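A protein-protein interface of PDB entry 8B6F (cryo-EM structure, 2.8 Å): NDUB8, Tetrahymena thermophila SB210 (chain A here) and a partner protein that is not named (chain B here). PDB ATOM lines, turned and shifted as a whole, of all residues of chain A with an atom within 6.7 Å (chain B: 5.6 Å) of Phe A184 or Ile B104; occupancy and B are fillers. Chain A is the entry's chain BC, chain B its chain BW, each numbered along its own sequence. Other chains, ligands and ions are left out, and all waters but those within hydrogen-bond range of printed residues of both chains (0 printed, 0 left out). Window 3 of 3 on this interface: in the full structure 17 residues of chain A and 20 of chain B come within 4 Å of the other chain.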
ATOM      1  N   ILE A 177      16.042 -30.881 -17.978  1.00  0.00           N
ATOM      2  CA  ILE A 177      16.072 -29.610 -17.260  1.00  0.00           C
ATOM      3  C   ILE A 177      17.479 -29.030 -17.266  1.00  0.00           C
ATOM      4  O   ILE A 177      17.670 -27.829 -17.491  1.00  0.00           O
ATOM      5  CB  ILE A 177      15.538 -29.799 -15.828  1.00  0.00           C
ATOM      6  CG1 ILE A 177      14.037 -30.099 -15.862  1.00  0.00           C
ATOM      7  CG2 ILE A 177      15.820 -28.570 -14.973  1.00  0.00           C
ATOM      8  CD1 ILE A 177      13.480 -30.597 -14.549  1.00  0.00           C
ATOM      9  N   ASN A 178      18.486 -29.863 -17.008  1.00  0.00           N
ATOM     10  CA  ASN A 178      19.862 -29.382 -17.042  1.00  0.00           C
ATOM     11  C   ASN A 178      20.231 -28.870 -18.428  1.00  0.00           C
ATOM     12  O   ASN A 178      20.866 -27.819 -18.561  1.00  0.00           O
ATOM     13  CB  ASN A 178      20.817 -30.496 -16.615  1.00  0.00           C
ATOM     14  CG  ASN A 178      20.651 -30.881 -15.160  1.00  0.00           C
ATOM     15  OD1 ASN A 178      20.316 -30.051 -14.319  1.00  0.00           O
ATOM     16  ND2 ASN A 178      20.883 -32.152 -14.858  1.00  0.00           N
ATOM     17  N   LEU A 179      19.842 -29.601 -19.475  1.00  0.00           N
ATOM     18  CA  LEU A 179      20.149 -29.166 -20.834  1.00  0.00           C
ATOM     19  C   LEU A 179      19.470 -27.841 -21.156  1.00  0.00           C
ATOM     20  O   LEU A 179      20.068 -26.967 -21.794  1.00  0.00           O
ATOM     21  CB  LEU A 179      19.726 -30.242 -21.835  1.00  0.00           C
ATOM     22  CG  LEU A 179      19.968 -29.922 -23.311  1.00  0.00           C
ATOM     23  CD1 LEU A 179      21.437 -29.649 -23.583  1.00  0.00           C
ATOM     24  CD2 LEU A 179      19.469 -31.059 -24.183  1.00  0.00           C
ATOM     25  N   GLU A 180      18.219 -27.675 -20.725  1.00  0.00           N
ATOM     26  CA  GLU A 180      17.516 -26.418 -20.960  1.00  0.00           C
ATOM     27  C   GLU A 180      18.185 -25.266 -20.224  1.00  0.00           C
ATOM     28  O   GLU A 180      18.272 -24.150 -20.749  1.00  0.00           O
ATOM     29  CB  GLU A 180      16.054 -26.550 -20.538  1.00  0.00           C
ATOM     30  CG  GLU A 180      15.237 -27.449 -21.450  1.00  0.00           C
ATOM     31  CD  GLU A 180      13.805 -27.607 -20.982  1.00  0.00           C
ATOM     32  OE1 GLU A 180      13.471 -27.077 -19.902  1.00  0.00           O
ATOM     33  OE2 GLU A 180      13.014 -28.261 -21.691  1.00  0.00           O
ATOM     34  N   ALA A 181      18.659 -25.511 -19.001  1.00  0.00           N
ATOM     35  CA  ALA A 181      19.386 -24.475 -18.278  1.00  0.00           C
ATOM     36  C   ALA A 181      20.661 -24.091 -19.014  1.00  0.00           C
ATOM     37  O   ALA A 181      20.997 -22.905 -19.115  1.00  0.00           O
ATOM     38  CB  ALA A 181      19.706 -24.948 -16.861  1.00  0.00           C
ATOM     39  N   LYS A 182      21.389 -25.080 -19.533  1.00  0.00           N
ATOM     40  CA  LYS A 182      22.589 -24.785 -20.305  1.00  0.00           C
ATOM     41  C   LYS A 182      22.251 -23.960 -21.540  1.00  0.00           C
ATOM     42  O   LYS A 182      22.948 -22.992 -21.861  1.00  0.00           O
ATOM     43  CB  LYS A 182      23.289 -26.085 -20.700  1.00  0.00           C
ATOM     44  CG  LYS A 182      24.508 -25.890 -21.589  1.00  0.00           C
ATOM     45  CD  LYS A 182      25.197 -27.212 -21.874  1.00  0.00           C
ATOM     46  CE  LYS A 182      26.414 -27.014 -22.758  1.00  0.00           C
ATOM     47  NZ  LYS A 182      27.133 -28.292 -23.005  1.00  0.00           N
ATOM     48  N   ASN A 183      21.186 -24.333 -22.249  1.00  0.00           N
ATOM     49  CA  ASN A 183      20.773 -23.566 -23.420  1.00  0.00           C
ATOM     50  C   ASN A 183      20.407 -22.139 -23.039  1.00  0.00           C
ATOM     51  O   ASN A 183      20.725 -21.193 -23.766  1.00  0.00           O
ATOM     52  CB  ASN A 183      19.597 -24.253 -24.112  1.00  0.00           C
ATOM     53  CG  ASN A 183      19.980 -25.582 -24.725  1.00  0.00           C
ATOM     54  OD1 ASN A 183      21.130 -25.795 -25.104  1.00  0.00           O
ATOM     55  ND2 ASN A 183      19.013 -26.486 -24.830  1.00  0.00           N
ATOM     56  N   PHE A 184      19.736 -21.964 -21.898  1.00  0.00           N
ATOM     57  CA  PHE A 184      19.379 -20.621 -21.454  1.00  0.00           C
ATOM     58  C   PHE A 184      20.614 -19.772 -21.185  1.00  0.00           C
ATOM     59  O   PHE A 184      20.671 -18.607 -21.593  1.00  0.00           O
ATOM     60  CB  PHE A 184      18.513 -20.699 -20.198  1.00  0.00           C
ATOM     61  CG  PHE A 184      18.588 -19.470 -19.339  1.00  0.00           C
ATOM     62  CD1 PHE A 184      17.890 -18.325 -19.685  1.00  0.00           C
ATOM     63  CD2 PHE A 184      19.351 -19.462 -18.185  1.00  0.00           C
ATOM     64  CE1 PHE A 184      17.956 -17.192 -18.898  1.00  0.00           C
ATOM     65  CE2 PHE A 184      19.422 -18.333 -17.391  1.00  0.00           C
ATOM     66  CZ  PHE A 184      18.722 -17.197 -17.748  1.00  0.00           C
ATOM     67  N   ILE A 185      21.616 -20.331 -20.508  1.00  0.00           N
ATOM     68  CA  ILE A 185      22.806 -19.543 -20.202  1.00  0.00           C
ATOM     69  C   ILE A 185      23.546 -19.186 -21.485  1.00  0.00           C
ATOM     70  O   ILE A 185      24.068 -18.076 -21.626  1.00  0.00           O
ATOM     71  CB  ILE A 185      23.706 -20.291 -19.197  1.00  0.00           C
ATOM     72  CG1 ILE A 185      24.424 -19.301 -18.277  1.00  0.00           C
ATOM     73  CG2 ILE A 185      24.748 -21.157 -19.897  1.00  0.00           C
ATOM     74  CD1 ILE A 185      23.511 -18.575 -17.306  1.00  0.00           C
ATOM     75  N   GLU A 186      23.612 -20.121 -22.436  1.00  0.00           N
ATOM     76  CA  GLU A 186      24.242 -19.817 -23.715  1.00  0.00           C
ATOM     77  C   GLU A 186      23.489 -18.712 -24.445  1.00  0.00           C
ATOM     78  O   GLU A 186      24.102 -17.801 -25.011  1.00  0.00           O
ATOM     79  CB  GLU A 186      24.313 -21.075 -24.579  1.00  0.00           C
ATOM     80  CG  GLU A 186      25.237 -22.147 -24.030  1.00  0.00           C
ATOM     81  CD  GLU A 186      25.241 -23.402 -24.880  1.00  0.00           C
ATOM     82  OE1 GLU A 186      24.480 -23.451 -25.870  1.00  0.00           O
ATOM     83  OE2 GLU A 186      26.004 -24.337 -24.559  1.00  0.00           O
ATOM     84  N   ARG A 187      22.156 -18.775 -24.439  1.00  0.00           N
ATOM     85  CA  ARG A 187      21.368 -17.744 -25.105  1.00  0.00           C
ATOM     86  C   ARG A 187      21.583 -16.384 -24.455  1.00  0.00           C
ATOM     87  O   ARG A 187      21.696 -15.367 -25.148  1.00  0.00           O
ATOM     88  CB  ARG A 187      19.886 -18.116 -25.080  1.00  0.00           C
ATOM     89  CG  ARG A 187      19.028 -17.273 -26.008  1.00  0.00           C
ATOM     90  CD  ARG A 187      17.545 -17.435 -25.716  1.00  0.00           C
ATOM     91  NE  ARG A 187      17.182 -18.820 -25.438  1.00  0.00           N
ATOM     92  CZ  ARG A 187      16.970 -19.320 -24.227  1.00  0.00           C
ATOM     93  NH1 ARG A 187      17.066 -18.574 -23.138  1.00  0.00           N
ATOM     94  NH2 ARG A 187      16.651 -20.606 -24.104  1.00  0.00           N
ATOM     95  N   VAL A 188      21.639 -16.344 -23.123  1.00  0.00           N
ATOM     96  CA  VAL A 188      21.871 -15.078 -22.432  1.00  0.00           C
ATOM     97  C   VAL A 188      23.238 -14.517 -22.797  1.00  0.00           C
ATOM     98  O   VAL A 188      23.383 -13.314 -23.047  1.00  0.00           O
ATOM     99  CB  VAL A 188      21.720 -15.267 -20.911  1.00  0.00           C
ATOM    100  CG1 VAL A 188      22.239 -14.050 -20.153  1.00  0.00           C
ATOM    101  CG2 VAL A 188      20.267 -15.528 -20.554  1.00  0.00           C
ATOM    102  N   GLU A 189      24.261 -15.371 -22.829  1.00  0.00           N
ATOM    103  CA  GLU A 189      25.589 -14.904 -23.208  1.00  0.00           C
ATOM    104  C   GLU A 189      25.587 -14.342 -24.623  1.00  0.00           C
ATOM    105  O   GLU A 189      26.159 -13.277 -24.877  1.00  0.00           O
ATOM    106  CB  GLU A 189      26.598 -16.045 -23.088  1.00  0.00           C
ATOM    107  CG  GLU A 189      28.031 -15.641 -23.403  1.00  0.00           C
ATOM    108  CD  GLU A 189      28.983 -16.818 -23.391  1.00  0.00           C
ATOM    109  OE1 GLU A 189      28.539 -17.939 -23.067  1.00  0.00           O
ATOM    110  OE2 GLU A 189      30.175 -16.625 -23.709  1.00  0.00           O
ATOM    111  N   VAL B  88      18.806 -24.494 -10.951  1.00  0.00           N
ATOM    112  CA  VAL B  88      17.611 -23.971 -11.605  1.00  0.00           C
ATOM    113  C   VAL B  88      16.494 -23.741 -10.598  1.00  0.00           C
ATOM    114  O   VAL B  88      15.757 -22.756 -10.692  1.00  0.00           O
ATOM    115  CB  VAL B  88      17.159 -24.926 -12.726  1.00  0.00           C
ATOM    116  CG1 VAL B  88      16.008 -24.318 -13.509  1.00  0.00           C
ATOM    117  CG2 VAL B  88      18.315 -25.258 -13.650  1.00  0.00           C
ATOM    118  N   ALA B  91      17.080 -20.492  -8.788  1.00  0.00           N
ATOM    119  CA  ALA B  91      16.765 -19.342  -9.628  1.00  0.00           C
ATOM    120  C   ALA B  91      15.260 -19.124  -9.711  1.00  0.00           C
ATOM    121  O   ALA B  91      14.783 -17.988  -9.611  1.00  0.00           O
ATOM    122  CB  ALA B  91      17.357 -19.531 -11.024  1.00  0.00           C
ATOM    123  N   TYR B  92      14.495 -20.200  -9.897  1.00  0.00           N
ATOM    124  CA  TYR B  92      13.043 -20.075  -9.936  1.00  0.00           C
ATOM    125  C   TYR B  92      12.499 -19.578  -8.604  1.00  0.00           C
ATOM    126  O   TYR B  92      11.578 -18.753  -8.568  1.00  0.00           O
ATOM    127  CB  TYR B  92      12.407 -21.412 -10.313  1.00  0.00           C
ATOM    128  CG  TYR B  92      12.150 -21.550 -11.793  1.00  0.00           C
ATOM    129  CD1 TYR B  92      13.141 -22.001 -12.653  1.00  0.00           C
ATOM    130  CD2 TYR B  92      10.915 -21.218 -12.331  1.00  0.00           C
ATOM    131  CE1 TYR B  92      12.907 -22.122 -14.007  1.00  0.00           C
ATOM    132  CE2 TYR B  92      10.671 -21.335 -13.681  1.00  0.00           C
ATOM    133  CZ  TYR B  92      11.670 -21.787 -14.515  1.00  0.00           C
ATOM    134  OH  TYR B  92      11.425 -21.904 -15.861  1.00  0.00           O
ATOM    135  N   ALA B  99      11.949 -15.818 -14.307  1.00  0.00           N
ATOM    136  CA  ALA B  99      12.322 -17.107 -14.874  1.00  0.00           C
ATOM    137  C   ALA B  99      11.344 -17.531 -15.961  1.00  0.00           C
ATOM    138  O   ALA B  99      11.757 -17.988 -17.030  1.00  0.00           O
ATOM    139  CB  ALA B  99      12.394 -18.164 -13.775  1.00  0.00           C
ATOM    140  N   ASP B 102      11.938 -15.293 -19.172  1.00  0.00           N
ATOM    141  CA  ASP B 102      13.021 -15.880 -19.962  1.00  0.00           C
ATOM    142  C   ASP B 102      13.261 -17.287 -19.423  1.00  0.00           C
ATOM    143  O   ASP B 102      14.179 -17.531 -18.639  1.00  0.00           O
ATOM    144  CB  ASP B 102      14.308 -15.003 -19.916  1.00  0.00           C
ATOM    145  CG  ASP B 102      14.850 -14.815 -18.509  1.00  0.00           C
ATOM    146  OD1 ASP B 102      14.238 -15.326 -17.551  1.00  0.00           O
ATOM    147  OD2 ASP B 102      15.899 -14.154 -18.360  1.00  0.00           O
ATOM    148  N   GLY B 103      12.422 -18.223 -19.866  1.00  0.00           N
ATOM    149  CA  GLY B 103      12.419 -19.570 -19.332  1.00  0.00           C
ATOM    150  C   GLY B 103      13.784 -20.214 -19.253  1.00  0.00           C
ATOM    151  O   GLY B 103      14.400 -20.534 -20.273  1.00  0.00           O
ATOM    152  N   ILE B 104      14.262 -20.411 -18.023  1.00  0.00           N
ATOM    153  CA  ILE B 104      15.495 -21.159 -17.819  1.00  0.00           C
ATOM    154  C   ILE B 104      15.293 -22.613 -18.217  1.00  0.00           C
ATOM    155  O   ILE B 104      16.134 -23.210 -18.898  1.00  0.00           O
ATOM    156  CB  ILE B 104      15.959 -21.026 -16.356  1.00  0.00           C
ATOM    157  CG1 ILE B 104      16.148 -19.547 -15.996  1.00  0.00           C
ATOM    158  CG2 ILE B 104      17.244 -21.815 -16.130  1.00  0.00           C
ATOM    159  CD1 ILE B 104      16.503 -19.296 -14.543  1.00  0.00           C
ATOM    160  N   SER B 105      14.173 -23.202 -17.799  1.00  0.00           N
ATOM    161  CA  SER B 105      13.819 -24.565 -18.188  1.00  0.00           C
ATOM    162  C   SER B 105      12.300 -24.672 -18.099  1.00  0.00           C
ATOM    163  O   SER B 105      11.748 -24.783 -17.000  1.00  0.00           O
ATOM    164  CB  SER B 105      14.506 -25.592 -17.299  1.00  0.00           C
ATOM    165  OG  SER B 105      14.107 -25.435 -15.947  1.00  0.00           O
ATOM    166  N   ASN B 106      11.632 -24.632 -19.253  1.00  0.00           N
ATOM    167  CA  ASN B 106      10.176 -24.712 -19.256  1.00  0.00           C
ATOM    168  C   ASN B 106       9.684 -25.997 -18.603  1.00  0.00           C
ATOM    169  O   ASN B 106       8.597 -26.016 -18.014  1.00  0.00           O
ATOM    170  CB  ASN B 106       9.649 -24.612 -20.686  1.00  0.00           C
ATOM    171  CG  ASN B 106       9.918 -23.259 -21.310  1.00  0.00           C
ATOM    172  OD1 ASN B 106       9.841 -22.230 -20.640  1.00  0.00           O
ATOM    173  ND2 ASN B 106      10.243 -23.254 -22.596  1.00  0.00           N
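The side-chain carboxylate of Glu A180 is in hydrogen-bond range of the backbone NH of Asn B106, at 3.1 Å. The backbone carbonyl oxygen of Ile B104 lies close to the backbone carbonyl oxygen of Glu A180, at 3.0 Å. O of Ile B104 is in hydrogen-bond range of N of Ala A181, 3.4 Å away.
The side-chain hydroxyl of Tyr B92 is in hydrogen-bond range of the backbone carbonyl oxygen of Ser B105.
Of the 13 printed residues of chain A, 4 touch a printed residue of chain B. Hydrophobic or aromatic side chains of chain A within 4 Å of the printed part of chain B: Ile A177, Ala A181 and Phe A184. Hydrophobic or aromatic side chains of chain B that line the printed part of chain A: Val B88 and Ile B104. Along chain B the printed residues that touch a printed residue of chain A span positions 88 to 106. Among the printed residues, 8 pairs touch across the chains.
CG2 of Ile A177 touches OG of Ser B105, 3.7 Å away. Glu A180 touches Ser B105 (OE1 to CA, 3.1 Å). Val B88 touches Ala A181 (CG2 to CB, 3.5 Å). Asp B102 touches Phe A184 (OD2 to CE1, 3.7 Å). CB of Phe A184 touches O of Ile B104, 3.7 Å away.
Printed residues of chain A within 4 Å of Ile B104: Glu A180 (3.0 Å), Ala A181 (3.4 Å) and Phe A184 (3.7 Å). Printed residues of chain B within 4 Å of Ala A181: Val B88 and Ile B104. Of the printed residues of chain A, Ser B105 touches Ile A177 (3.7 Å) and Glu A180 (3.1 Å).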
